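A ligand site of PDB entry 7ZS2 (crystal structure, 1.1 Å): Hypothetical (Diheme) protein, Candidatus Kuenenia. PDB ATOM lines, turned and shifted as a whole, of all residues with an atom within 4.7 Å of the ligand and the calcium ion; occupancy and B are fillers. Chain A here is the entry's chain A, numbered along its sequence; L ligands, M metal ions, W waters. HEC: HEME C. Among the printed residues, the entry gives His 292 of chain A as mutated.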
ATOM      1  N   ARG A  70      11.029   9.437  -5.329  1.00  0.00           N
ATOM      2  CA  ARG A  70      10.547  10.767  -4.993  1.00  0.00           C
ATOM      3  C   ARG A  70      10.242  11.588  -6.229  1.00  0.00           C
ATOM      4  O   ARG A  70       9.329  12.419  -6.193  1.00  0.00           O
ATOM      5  CB  ARG A  70      11.528  11.531  -4.097  1.00  0.00           C
ATOM      6  CG  ARG A  70      11.424  11.296  -2.601  1.00  0.00           C
ATOM      7  CD  ARG A  70      12.503  11.971  -1.841  1.00  0.00           C
ATOM      8  NE  ARG A  70      12.490  11.691  -0.393  1.00  0.00           N
ATOM      9  CZ  ARG A  70      13.070  10.628   0.144  1.00  0.00           C
ATOM     10  NH1 ARG A  70      13.607   9.682  -0.602  1.00  0.00           N
ATOM     11  NH2 ARG A  70      13.094  10.487   1.467  1.00  0.00           N
ATOM     12  N   ILE A 115       9.143  19.356  -4.636  1.00  0.00           N
ATOM     13  CA  ILE A 115      10.182  18.775  -3.782  1.00  0.00           C
ATOM     14  C   ILE A 115      11.583  18.945  -4.378  1.00  0.00           C
ATOM     15  O   ILE A 115      12.569  18.907  -3.643  1.00  0.00           O
ATOM     16  CB  ILE A 115       9.851  17.321  -3.445  1.00  0.00           C
ATOM     17  CG1 ILE A 115      10.674  16.744  -2.284  1.00  0.00           C
ATOM     18  CG2 ILE A 115       9.960  16.416  -4.686  1.00  0.00           C
ATOM     19  CD1 ILE A 115      10.153  15.407  -1.749  1.00  0.00           C
ATOM     20  N   PHE A 183      14.756  14.854  18.323  1.00  0.00           N
ATOM     21  CA  PHE A 183      14.159  14.015  17.273  1.00  0.00           C
ATOM     22  C   PHE A 183      13.703  12.669  17.810  1.00  0.00           C
ATOM     23  O   PHE A 183      12.657  12.145  17.394  1.00  0.00           O
ATOM     24  CB  PHE A 183      15.215  13.847  16.150  1.00  0.00           C
ATOM     25  CG  PHE A 183      14.735  13.222  14.883  1.00  0.00           C
ATOM     26  CD1 PHE A 183      14.617  11.856  14.766  1.00  0.00           C
ATOM     27  CD2 PHE A 183      14.421  13.981  13.783  1.00  0.00           C
ATOM     28  CE1 PHE A 183      14.256  11.265  13.593  1.00  0.00           C
ATOM     29  CE2 PHE A 183      14.044  13.417  12.607  1.00  0.00           C
ATOM     30  CZ  PHE A 183      13.972  12.047  12.510  1.00  0.00           C
ATOM     31  N   VAL A 190       5.547  15.268  20.434  1.00  0.00           N
ATOM     32  CA  VAL A 190       5.826  14.704  19.120  1.00  0.00           C
ATOM     33  C   VAL A 190       7.205  14.101  19.205  1.00  0.00           C
ATOM     34  O   VAL A 190       8.097  14.697  19.796  1.00  0.00           O
ATOM     35  CB  VAL A 190       5.707  15.762  18.000  1.00  0.00           C
ATOM     36  CG1 VAL A 190       6.683  16.938  18.217  1.00  0.00           C
ATOM     37  CG2 VAL A 190       5.923  15.104  16.609  1.00  0.00           C
ATOM     38  N   THR A 191       7.379  12.930  18.585  1.00  0.00           N
ATOM     39  CA  THR A 191       8.665  12.263  18.505  1.00  0.00           C
ATOM     40  C   THR A 191       8.881  11.930  17.037  1.00  0.00           C
ATOM     41  O   THR A 191       8.248  10.999  16.503  1.00  0.00           O
ATOM     42  CB  THR A 191       8.670  10.996  19.346  1.00  0.00           C
ATOM     43  OG1 THR A 191       8.280  11.320  20.694  1.00  0.00           O
ATOM     44  CG2 THR A 191      10.088  10.378  19.336  1.00  0.00           C
ATOM     45  N   CYS A 192       9.768  12.682  16.388  1.00  0.00           N
ATOM     46  CA  CYS A 192      10.000  12.422  14.963  1.00  0.00           C
ATOM     47  C   CYS A 192      10.371  10.975  14.716  1.00  0.00           C
ATOM     48  O   CYS A 192       9.986  10.402  13.684  1.00  0.00           O
ATOM     49  CB  CYS A 192      11.101  13.310  14.379  1.00  0.00           C
ATOM     50  SG  CYS A 192      11.015  15.057  14.869  1.00  0.00           S
ATOM     51  N   CYS A 195       8.219   8.025  13.530  1.00  0.00           N
ATOM     52  CA  CYS A 195       7.817   7.896  12.156  1.00  0.00           C
ATOM     53  C   CYS A 195       8.947   7.973  11.147  1.00  0.00           C
ATOM     54  O   CYS A 195       8.695   7.700   9.949  1.00  0.00           O
ATOM     55  CB  CYS A 195       6.832   8.998  11.789  1.00  0.00           C
ATOM     56  SG  CYS A 195       5.250   8.830  12.656  1.00  0.00           S
ATOM     57  N   HIS A 196      10.148   8.356  11.538  1.00  0.00           N
ATOM     58  CA  HIS A 196      11.235   8.491  10.597  1.00  0.00           C
ATOM     59  C   HIS A 196      12.475   7.820  11.158  1.00  0.00           C
ATOM     60  O   HIS A 196      12.850   8.035  12.318  1.00  0.00           O
ATOM     61  CB  HIS A 196      11.570   9.987  10.404  1.00  0.00           C
ATOM     62  CG  HIS A 196      10.527  10.778   9.708  1.00  0.00           C
ATOM     63  ND1 HIS A 196      10.310  10.702   8.343  1.00  0.00           N
ATOM     64  CD2 HIS A 196       9.649  11.708  10.158  1.00  0.00           C
ATOM     65  CE1 HIS A 196       9.384  11.579   8.016  1.00  0.00           C
ATOM     66  NE2 HIS A 196       8.942  12.207   9.095  1.00  0.00           N
ATOM     67  N   VAL A 205       7.482   5.076   9.360  1.00  0.00           N
ATOM     68  CA  VAL A 205       6.130   5.413   8.954  1.00  0.00           C
ATOM     69  C   VAL A 205       6.243   6.319   7.735  1.00  0.00           C
ATOM     70  O   VAL A 205       5.797   5.960   6.642  1.00  0.00           O
ATOM     71  CB  VAL A 205       5.348   6.076  10.105  1.00  0.00           C
ATOM     72  CG1 VAL A 205       3.958   6.587   9.610  1.00  0.00           C
ATOM     73  CG2 VAL A 205       5.173   5.185  11.314  1.00  0.00           C
ATOM     74  N   GLY A 206       6.844   7.494   7.908  1.00  0.00           N
ATOM     75  CA  GLY A 206       7.303   8.282   6.786  1.00  0.00           C
ATOM     76  C   GLY A 206       8.663   7.842   6.296  1.00  0.00           C
ATOM     77  O   GLY A 206       9.195   6.836   6.743  1.00  0.00           O
ATOM     78  N   PRO A 207       9.208   8.577   5.351  1.00  0.00           N
ATOM     79  CA  PRO A 207      10.443   8.151   4.704  1.00  0.00           C
ATOM     80  C   PRO A 207      11.645   8.239   5.640  1.00  0.00           C
ATOM     81  O   PRO A 207      11.719   9.086   6.550  1.00  0.00           O
ATOM     82  CB  PRO A 207      10.595   9.120   3.545  1.00  0.00           C
ATOM     83  CG  PRO A 207       9.762  10.280   3.921  1.00  0.00           C
ATOM     84  CD  PRO A 207       8.587   9.724   4.679  1.00  0.00           C
ATOM     85  N   LEU A 209      15.141   9.502   6.691  1.00  0.00           N
ATOM     86  CA  LEU A 209      15.696  10.837   6.531  1.00  0.00           C
ATOM     87  C   LEU A 209      17.214  10.852   6.435  1.00  0.00           C
ATOM     88  O   LEU A 209      17.808  11.888   6.180  1.00  0.00           O
ATOM     89  CB  LEU A 209      15.203  11.808   7.623  1.00  0.00           C
ATOM     90  CG  LEU A 209      13.694  11.979   7.637  1.00  0.00           C
ATOM     91  CD1 LEU A 209      13.321  12.988   8.736  1.00  0.00           C
ATOM     92  CD2 LEU A 209      13.106  12.442   6.328  1.00  0.00           C
ATOM     93  N   ILE A 212      19.320  13.357   4.075  1.00  0.00           N
ATOM     94  CA  ILE A 212      18.512  14.452   3.509  1.00  0.00           C
ATOM     95  C   ILE A 212      19.190  15.811   3.644  1.00  0.00           C
ATOM     96  O   ILE A 212      18.892  16.737   2.876  1.00  0.00           O
ATOM     97  CB  ILE A 212      17.094  14.439   4.120  1.00  0.00           C
ATOM     98  CG1 ILE A 212      16.125  15.212   3.229  1.00  0.00           C
ATOM     99  CG2 ILE A 212      17.082  14.958   5.562  1.00  0.00           C
ATOM    100  CD1 ILE A 212      14.662  15.070   3.607  1.00  0.00           C
ATOM    101  N   TYR A 220      12.957  23.946   3.200  1.00  0.00           N
ATOM    102  CA  TYR A 220      12.175  22.756   2.967  1.00  0.00           C
ATOM    103  C   TYR A 220      11.918  22.015   4.283  1.00  0.00           C
ATOM    104  O   TYR A 220      10.848  21.446   4.481  1.00  0.00           O
ATOM    105  CB  TYR A 220      12.855  21.846   1.929  1.00  0.00           C
ATOM    106  CG  TYR A 220      12.083  20.566   1.721  1.00  0.00           C
ATOM    107  CD1 TYR A 220      10.901  20.548   1.006  1.00  0.00           C
ATOM    108  CD2 TYR A 220      12.483  19.360   2.309  1.00  0.00           C
ATOM    109  CE1 TYR A 220      10.191  19.390   0.803  1.00  0.00           C
ATOM    110  CE2 TYR A 220      11.765  18.204   2.130  1.00  0.00           C
ATOM    111  CZ  TYR A 220      10.615  18.203   1.403  1.00  0.00           C
ATOM    112  OH  TYR A 220       9.857  17.085   1.189  1.00  0.00           O
ATOM    113  N   PHE A 221      12.899  21.997   5.171  1.00  0.00           N
ATOM    114  CA  PHE A 221      12.696  21.386   6.480  1.00  0.00           C
ATOM    115  C   PHE A 221      11.634  22.124   7.283  1.00  0.00           C
ATOM    116  O   PHE A 221      10.778  21.501   7.900  1.00  0.00           O
ATOM    117  CB  PHE A 221      13.997  21.254   7.261  1.00  0.00           C
ATOM    118  CG  PHE A 221      15.053  20.405   6.579  1.00  0.00           C
ATOM    119  CD1 PHE A 221      14.735  19.260   5.872  1.00  0.00           C
ATOM    120  CD2 PHE A 221      16.389  20.736   6.669  1.00  0.00           C
ATOM    121  CE1 PHE A 221      15.708  18.532   5.237  1.00  0.00           C
ATOM    122  CE2 PHE A 221      17.369  20.000   6.033  1.00  0.00           C
ATOM    123  CZ  PHE A 221      17.021  18.885   5.318  1.00  0.00           C
ATOM    124  N   SER A 224       8.342  21.300   5.738  1.00  0.00           N
ATOM    125  CA  SER A 224       7.992  19.919   5.959  1.00  0.00           C
ATOM    126  C   SER A 224       7.488  19.708   7.386  1.00  0.00           C
ATOM    127  O   SER A 224       6.581  18.896   7.626  1.00  0.00           O
ATOM    128  CB  SER A 224       9.200  19.008   5.736  1.00  0.00           C
ATOM    129  OG  SER A 224       9.529  18.905   4.368  1.00  0.00           O
ATOM    130  N   ILE A 225       8.082  20.398   8.352  1.00  0.00           N
ATOM    131  CA  ILE A 225       7.711  20.204   9.740  1.00  0.00           C
ATOM    132  C   ILE A 225       6.377  20.867  10.038  1.00  0.00           C
ATOM    133  O   ILE A 225       5.519  20.262  10.692  1.00  0.00           O
ATOM    134  CB  ILE A 225       8.815  20.674  10.691  1.00  0.00           C
ATOM    135  CG1 ILE A 225      10.058  19.821  10.535  1.00  0.00           C
ATOM    136  CG2 ILE A 225       8.320  20.698  12.131  1.00  0.00           C
ATOM    137  CD1 ILE A 225      11.306  20.409  11.196  1.00  0.00           C
ATOM    138  N   PRO A 228       2.942  20.162   6.674  1.00  0.00           N
ATOM    139  CA  PRO A 228       3.268  18.828   6.129  1.00  0.00           C
ATOM    140  C   PRO A 228       2.591  18.447   4.856  1.00  0.00           C
ATOM    141  O   PRO A 228       3.136  17.630   4.119  1.00  0.00           O
ATOM    142  CB  PRO A 228       2.828  17.876   7.271  1.00  0.00           C
ATOM    143  CG  PRO A 228       1.844  18.698   8.076  1.00  0.00           C
ATOM    144  CD  PRO A 228       2.431  20.087   8.056  1.00  0.00           C
ATOM    145  N   SER A 229       1.400  18.987   4.569  1.00  0.00           N
ATOM    146  CA  SER A 229       0.703  18.618   3.358  1.00  0.00           C
ATOM    147  C   SER A 229       1.058  19.528   2.173  1.00  0.00           C
ATOM    148  O   SER A 229       0.566  19.280   1.063  1.00  0.00           O
ATOM    149  CB  SER A 229      -0.817  18.570   3.612  1.00  0.00           C
ATOM    150  OG  SER A 229      -1.101  17.617   4.639  1.00  0.00           O
ATOM    151  N   VAL A 231       3.894  19.549   0.563  1.00  0.00           N
ATOM    152  CA  VAL A 231       4.608  18.609  -0.310  1.00  0.00           C
ATOM    153  C   VAL A 231       4.336  17.252   0.285  1.00  0.00           C
ATOM    154  O   VAL A 231       4.590  17.057   1.470  1.00  0.00           O
ATOM    155  CB  VAL A 231       6.121  18.863  -0.335  1.00  0.00           C
ATOM    156  CG1 VAL A 231       6.892  17.682  -1.024  1.00  0.00           C
ATOM    157  CG2 VAL A 231       6.424  20.177  -0.980  1.00  0.00           C
ATOM    158  N   ILE A 232       3.846  16.309  -0.506  1.00  0.00           N
ATOM    159  CA  ILE A 232       3.660  14.931  -0.036  1.00  0.00           C
ATOM    160  C   ILE A 232       4.686  14.078  -0.763  1.00  0.00           C
ATOM    161  O   ILE A 232       4.586  13.906  -2.002  1.00  0.00           O
ATOM    162  CB  ILE A 232       2.251  14.425  -0.326  1.00  0.00           C
ATOM    163  CG1 ILE A 232       1.143  15.238   0.373  1.00  0.00           C
ATOM    164  CG2 ILE A 232       2.181  12.938   0.055  1.00  0.00           C
ATOM    165  CD1 ILE A 232       1.120  15.133   1.914  1.00  0.00           C
ATOM    166  N   VAL A 233       5.622  13.512  -0.041  1.00  0.00           N
ATOM    167  CA  VAL A 233       6.602  12.593  -0.639  1.00  0.00           C
ATOM    168  C   VAL A 233       5.861  11.482  -1.367  1.00  0.00           C
ATOM    169  O   VAL A 233       4.964  10.832  -0.800  1.00  0.00           O
ATOM    170  CB  VAL A 233       7.531  12.069   0.453  1.00  0.00           C
ATOM    171  CG1 VAL A 233       8.505  11.027  -0.162  1.00  0.00           C
ATOM    172  CG2 VAL A 233       8.308  13.147   1.101  1.00  0.00           C
ATOM    173  N   TYR A 236       3.755   8.207  -0.051  1.00  0.00           N
ATOM    174  CA  TYR A 236       3.356   8.380   1.339  1.00  0.00           C
ATOM    175  C   TYR A 236       2.076   9.152   1.464  1.00  0.00           C
ATOM    176  O   TYR A 236       1.816   9.791   2.474  1.00  0.00           O
ATOM    177  CB  TYR A 236       4.486   9.038   2.139  1.00  0.00           C
ATOM    178  CG  TYR A 236       5.716   8.209   2.288  1.00  0.00           C
ATOM    179  CD1 TYR A 236       6.677   8.183   1.323  1.00  0.00           C
ATOM    180  CD2 TYR A 236       5.842   7.367   3.370  1.00  0.00           C
ATOM    181  CE1 TYR A 236       7.807   7.382   1.427  1.00  0.00           C
ATOM    182  CE2 TYR A 236       6.958   6.552   3.484  1.00  0.00           C
ATOM    183  CZ  TYR A 236       7.947   6.549   2.521  1.00  0.00           C
ATOM    184  OH  TYR A 236       9.004   5.742   2.674  1.00  0.00           O
ATOM    185  N   LEU A 252      -1.879   5.883   5.631  1.00  0.00           N
ATOM    186  CA  LEU A 252      -0.935   5.629   4.576  1.00  0.00           C
ATOM    187  C   LEU A 252      -0.760   4.138   4.357  1.00  0.00           C
ATOM    188  O   LEU A 252      -0.957   3.318   5.241  1.00  0.00           O
ATOM    189  CB  LEU A 252       0.352   6.455   4.610  1.00  0.00           C
ATOM    190  CG  LEU A 252       1.308   6.126   5.660  1.00  0.00           C
ATOM    191  CD1 LEU A 252       2.044   4.806   5.520  1.00  0.00           C
ATOM    192  CD2 LEU A 252       2.387   7.282   5.750  1.00  0.00           C
ATOM    193  N   GLU A 266      -2.995   7.470  11.895  1.00  0.00           N
ATOM    194  CA  GLU A 266      -2.411   8.382  12.855  1.00  0.00           C
ATOM    195  C   GLU A 266      -3.520   9.106  13.587  1.00  0.00           C
ATOM    196  O   GLU A 266      -4.532   9.484  13.003  1.00  0.00           O
ATOM    197  CB  GLU A 266      -1.470   9.388  12.189  1.00  0.00           C
ATOM    198  CG  GLU A 266      -0.764  10.331  13.062  1.00  0.00           C
ATOM    199  CD  GLU A 266      -1.567  11.574  13.493  1.00  0.00           C
ATOM    200  OE1 GLU A 266      -2.535  11.929  12.813  1.00  0.00           O
ATOM    201  OE2 GLU A 266      -1.204  12.128  14.527  1.00  0.00           O
ATOM    202  N   VAL A 271       0.558   6.226  16.160  1.00  0.00           N
ATOM    203  CA  VAL A 271       0.262   5.483  14.949  1.00  0.00           C
ATOM    204  C   VAL A 271      -0.210   4.073  15.321  1.00  0.00           C
ATOM    205  O   VAL A 271       0.105   3.549  16.391  1.00  0.00           O
ATOM    206  CB  VAL A 271       1.498   5.425  14.010  1.00  0.00           C
ATOM    207  CG1 VAL A 271       1.700   6.809  13.371  1.00  0.00           C
ATOM    208  CG2 VAL A 271       2.778   4.960  14.736  1.00  0.00           C
ATOM    209  N   SER A 290      -1.193  14.690   4.544  1.00  0.00           N
ATOM    210  CA  SER A 290      -0.130  13.887   5.114  1.00  0.00           C
ATOM    211  C   SER A 290      -0.503  13.368   6.500  1.00  0.00           C
ATOM    212  O   SER A 290      -1.164  14.064   7.270  1.00  0.00           O
ATOM    213  CB  SER A 290       1.119  14.776   5.272  1.00  0.00           C
ATOM    214  OG  SER A 290       2.177  14.039   5.830  1.00  0.00           O
ATOM    215  N   ILE A 291       0.047  12.191   6.860  1.00  0.00           N
ATOM    216  CA  ILE A 291      -0.074  11.757   8.260  1.00  0.00           C
ATOM    217  C   ILE A 291       0.917  12.418   9.172  1.00  0.00           C
ATOM    218  O   ILE A 291       0.754  12.334  10.388  1.00  0.00           O
ATOM    219  CB  ILE A 291      -0.238  10.265   8.514  1.00  0.00           C
ATOM    220  CG1 ILE A 291       0.986   9.587   8.345  1.00  0.00           C
ATOM    221  CG2 ILE A 291      -1.243   9.550   7.739  1.00  0.00           C
ATOM    222  CD1 ILE A 291       0.982   8.105   8.929  1.00  0.00           C
ATOM    223  N   HIS A 292       1.979  13.085   8.647  1.00  0.00           N
ATOM    224  CA  HIS A 292       2.852  13.884   9.499  1.00  0.00           C
ATOM    225  C   HIS A 292       1.974  14.917  10.183  1.00  0.00           C
ATOM    226  O   HIS A 292       1.247  15.638   9.483  1.00  0.00           O
ATOM    227  CB  HIS A 292       3.952  14.491   8.620  1.00  0.00           C
ATOM    228  CG  HIS A 292       4.871  15.430   9.302  1.00  0.00           C
ATOM    229  ND1 HIS A 292       6.260  15.356   9.212  1.00  0.00           N
ATOM    230  CD2 HIS A 292       4.580  16.627   9.880  1.00  0.00           C
ATOM    231  CE1 HIS A 292       6.735  16.476   9.724  1.00  0.00           C
ATOM    232  NE2 HIS A 292       5.743  17.241  10.154  1.00  0.00           N
ATOM    233  N   PRO A 293       1.988  15.062  11.515  1.00  0.00           N
ATOM    234  CA  PRO A 293       1.015  15.891  12.189  1.00  0.00           C
ATOM    235  C   PRO A 293       1.060  17.337  11.768  1.00  0.00           C
ATOM    236  O   PRO A 293       2.115  17.915  11.530  1.00  0.00           O
ATOM    237  CB  PRO A 293       1.408  15.747  13.680  1.00  0.00           C
ATOM    238  CG  PRO A 293       2.052  14.397  13.759  1.00  0.00           C
ATOM    239  CD  PRO A 293       2.756  14.258  12.479  1.00  0.00           C
ATOM    240  N   ILE A 296       2.683  20.583  14.846  1.00  0.00           N
ATOM    241  CA  ILE A 296       3.977  20.552  15.495  1.00  0.00           C
ATOM    242  C   ILE A 296       4.402  21.925  16.001  1.00  0.00           C
ATOM    243  O   ILE A 296       5.131  22.018  16.976  1.00  0.00           O
ATOM    244  CB  ILE A 296       5.006  19.872  14.585  1.00  0.00           C
ATOM    245  CG1 ILE A 296       4.519  18.422  14.397  1.00  0.00           C
ATOM    246  CG2 ILE A 296       6.417  19.985  15.166  1.00  0.00           C
ATOM    247  CD1 ILE A 296       5.347  17.616  13.435  1.00  0.00           C
ATOM    248  N   LEU A 300       6.401  21.789  19.775  1.00  0.00           N
ATOM    249  CA  LEU A 300       7.816  22.033  19.978  1.00  0.00           C
ATOM    250  C   LEU A 300       8.040  23.473  20.402  1.00  0.00           C
ATOM    251  O   LEU A 300       7.384  24.406  19.911  1.00  0.00           O
ATOM    252  CB  LEU A 300       8.605  21.745  18.735  1.00  0.00           C
ATOM    253  CG  LEU A 300       8.687  20.301  18.269  1.00  0.00           C
ATOM    254  CD1 LEU A 300       9.547  20.258  16.998  1.00  0.00           C
ATOM    255  CD2 LEU A 300       9.202  19.361  19.405  1.00  0.00           C
ATOM    256  N   VAL A 308      16.036  20.801  15.891  1.00  0.00           N
ATOM    257  CA  VAL A 308      15.731  19.715  14.946  1.00  0.00           C
ATOM    258  C   VAL A 308      16.124  20.082  13.537  1.00  0.00           C
ATOM    259  O   VAL A 308      16.619  19.246  12.802  1.00  0.00           O
ATOM    260  CB  VAL A 308      14.268  19.310  15.079  1.00  0.00           C
ATOM    261  CG1 VAL A 308      13.780  18.514  13.816  1.00  0.00           C
ATOM    262  CG2 VAL A 308      14.028  18.681  16.308  1.00  0.00           C
ATOM    263  N   LEU A 312      18.557  17.974  11.028  1.00  0.00           N
ATOM    264  CA  LEU A 312      18.285  17.566   9.657  1.00  0.00           C
ATOM    265  C   LEU A 312      19.368  18.040   8.697  1.00  0.00           C
ATOM    266  O   LEU A 312      19.777  17.304   7.815  1.00  0.00           O
ATOM    267  CB  LEU A 312      16.914  18.068   9.230  1.00  0.00           C
ATOM    268  CG  LEU A 312      15.726  17.479   9.961  1.00  0.00           C
ATOM    269  CD1 LEU A 312      14.482  18.207   9.639  1.00  0.00           C
ATOM    270  CD2 LEU A 312      15.576  16.005   9.630  1.00  0.00           C
HETATM  271 FE   HEC L   1       7.615  13.733   9.085  1.00  0.00          FE
HETATM  272  CHA HEC L   1       7.629  13.779   5.651  1.00  0.00           C
HETATM  273  CHB HEC L   1      10.392  15.676   9.131  1.00  0.00           C
HETATM  274  CHC HEC L   1       7.392  13.904  12.464  1.00  0.00           C
HETATM  275  CHD HEC L   1       5.301  11.238   9.059  1.00  0.00           C
HETATM  276  NA  HEC L   1       8.764  14.641   7.650  1.00  0.00           N
HETATM  277  C1A HEC L   1       8.615  14.502   6.293  1.00  0.00           C
HETATM  278  C2A HEC L   1       9.713  15.207   5.668  1.00  0.00           C
HETATM  279  C3A HEC L   1      10.474  15.736   6.627  1.00  0.00           C
HETATM  280  C4A HEC L   1       9.884  15.358   7.893  1.00  0.00           C
HETATM  281  CMA HEC L   1      11.770  16.522   6.486  1.00  0.00           C
HETATM  282  CAA HEC L   1       9.996  15.225   4.162  1.00  0.00           C
HETATM  283  CBA HEC L   1      10.938  14.075   3.809  1.00  0.00           C
HETATM  284  CGA HEC L   1      11.414  13.991   2.386  1.00  0.00           C
HETATM  285  O1A HEC L   1      11.895  12.926   1.999  1.00  0.00           O
HETATM  286  O2A HEC L   1      11.363  14.993   1.661  1.00  0.00           O
HETATM  287  NB  HEC L   1       8.697  14.605  10.512  1.00  0.00           N
HETATM  288  C1B HEC L   1       9.852  15.322  10.359  1.00  0.00           C
HETATM  289  C2B HEC L   1      10.308  15.805  11.626  1.00  0.00           C
HETATM  290  C3B HEC L   1       9.443  15.353  12.567  1.00  0.00           C
HETATM  291  C4B HEC L   1       8.429  14.612  11.887  1.00  0.00           C
HETATM  292  CMB HEC L   1      11.625  16.531  11.817  1.00  0.00           C
HETATM  293  CAB HEC L   1       9.511  15.583  14.058  1.00  0.00           C
HETATM  294  CBB HEC L   1       9.282  17.053  14.416  1.00  0.00           C
HETATM  295  NC  HEC L   1       6.530  12.781  10.485  1.00  0.00           N
HETATM  296  C1C HEC L   1       6.555  13.024  11.847  1.00  0.00           C
HETATM  297  C2C HEC L   1       5.631  12.156  12.506  1.00  0.00           C
HETATM  298  C3C HEC L   1       5.079  11.350  11.565  1.00  0.00           C
HETATM  299  C4C HEC L   1       5.627  11.737  10.271  1.00  0.00           C
HETATM  300  CMC HEC L   1       5.481  12.109  14.009  1.00  0.00           C
HETATM  301  CAC HEC L   1       4.250  10.094  11.742  1.00  0.00           C
HETATM  302  CBC HEC L   1       2.929  10.268  12.455  1.00  0.00           C
HETATM  303  ND  HEC L   1       6.624  12.769   7.645  1.00  0.00           N
HETATM  304  C1D HEC L   1       5.734  11.728   7.826  1.00  0.00           C
HETATM  305  C2D HEC L   1       5.273  11.235   6.588  1.00  0.00           C
HETATM  306  C3D HEC L   1       5.918  12.000   5.597  1.00  0.00           C
HETATM  307  C4D HEC L   1       6.763  12.915   6.278  1.00  0.00           C
HETATM  308  CMD HEC L   1       4.263  10.155   6.351  1.00  0.00           C
HETATM  309  CAD HEC L   1       5.758  11.839   4.104  1.00  0.00           C
HETATM  310  CBD HEC L   1       4.579  12.620   3.526  1.00  0.00           C
HETATM  311  CGD HEC L   1       4.853  14.098   3.574  1.00  0.00           C
HETATM  312  O1D HEC L   1       5.716  14.575   2.764  1.00  0.00           O
HETATM  313  O2D HEC L   1       4.294  14.843   4.413  1.00  0.00           O
HETATM  314 CA    CA M   1       5.330  16.909   3.594  1.00  0.00          CA
HETATM  315  O   HOH W   1      13.412  15.286  -0.219  1.00  0.00           O
HETATM  316  O   HOH W   2       5.405  19.369   3.513  1.00  0.00           O
HETATM  317  O   HOH W   3       7.611  17.378   2.907  1.00  0.00           O
HETATM  318  O   HOH W   4       6.153  16.891   5.843  1.00  0.00           O
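CAB of the ligand is covalently linked to SG of Cys 192 (1.8 Å).
The side-chain sulfur (SG) of Cys 195 is bonded to a carbon (CAC) of the ligand (1.9 Å).
A ring nitrogen (NE2) of His 196 is bound to an iron atom (FE) of the ligand (2.0 Å).
An iron atom (FE) of the ligand is bound by a ring nitrogen (ND1) of His 292, at 2.1 Å.
An oxygen (O2A) of the ligand lies within hydrogen-bond range of the side-chain hydroxyl (OH) of Tyr 220 (2.6 Å).
OG of Ser 290 lies close to O2D of the ligand (2.7 Å).
An oxygen (O1A) of the ligand is in salt-bridge range of the guanidinium group of Arg 70 (2.8 Å).
N of Val 233 sits close to O1D of the ligand, at 3.0 Å.
N of Cys 192 sits at hydrogen-bond distance from O of Phe 183 (3.1 Å).
The backbone carbonyl oxygen of Cys 195 sits at hydrogen-bond distance from the backbone NH of Gly 206, at 2.8 Å.
The backbone carbonyl oxygen (O) of Cys 195 lies within hydrogen-bond range of the backbone NH (N) of Val 205.
O of Pro 207 sits at hydrogen-bond distance from ND1 of His 196.
O of Ser 224 lies within hydrogen-bond range of NE2 of His 292, 3.1 Å away.
The backbone carbonyl oxygen (O) of Ile 225 sits at hydrogen-bond distance from a ring nitrogen (NE2) of His 292, 3.1 Å away.
The backbone carbonyl oxygen (O) of Tyr 220 is in hydrogen-bond range of the side-chain hydroxyl (OG) of Ser 224 (2.9 Å).
The backbone NH of Ser 290 is in hydrogen-bond range of the side-chain hydroxyl of Ser 229, at 2.9 Å.
Merely in contact with the ligand: Ile 115 (3.6 Å), Val 190 (3.99 Å), Thr 191 (3.9 Å), Gly 206 (3.6 Å), Pro 207 (3.6 Å), Leu 209 (3.7 Å), Ile 212 (3.6 Å), Ser 224 (3.6 Å), Ile 225 (3.9 Å), Ile 232 (3.5 Å), Tyr 236 (3.7 Å), Leu 252 (3.5 Å), Glu 266 (3.7 Å), Val 271 (3.8 Å), Ile 291 (3.6 Å), Pro 293 (3.6 Å), Val 308 (3.5 Å) and Leu 312 (3.96 Å).
28 residues have an atom within 4 Å of the ligand: Arg 70, Ile 115, Val 190, Thr 191, Cys 192, Cys 195, His 196, Gly 206, Pro 207, Leu 209, Ile 212, Tyr 220, Ser 224, Ile 225, Pro 228, Val 231, Ile 232, Val 233, Tyr 236, Leu 252, Glu 266, Val 271, Ser 290, Ile 291, His 292, Pro 293, Val 308 and Leu 312.
The nearest printed residue that does not touch the ligand is Phe 183 (4.02 Å).
Within 4 Å of the calcium ion: Pro 228 and Val 231.
The nearest printed residue that does not touch the calcium ion is Ile 232 (4.4 Å).
The calcium ion is bound by the backbone carbonyl oxygen (O) of Val 231 (2.3 Å), the backbone carbonyl oxygen (O) of Pro 228 (2.4 Å), water W4 (2.4 Å), water W3 (2.4 Å), an oxygen (O2D) of the ligand (2.5 Å), water W2 (2.5 Å) and an oxygen (O1D) of the ligand (2.5 Å).
The calcium ion has seven donor atoms within binding distance.
Water W3 lies within hydrogen-bond range of OH of Tyr 220 (2.8 Å) and OG of Ser 224 (2.9 Å).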
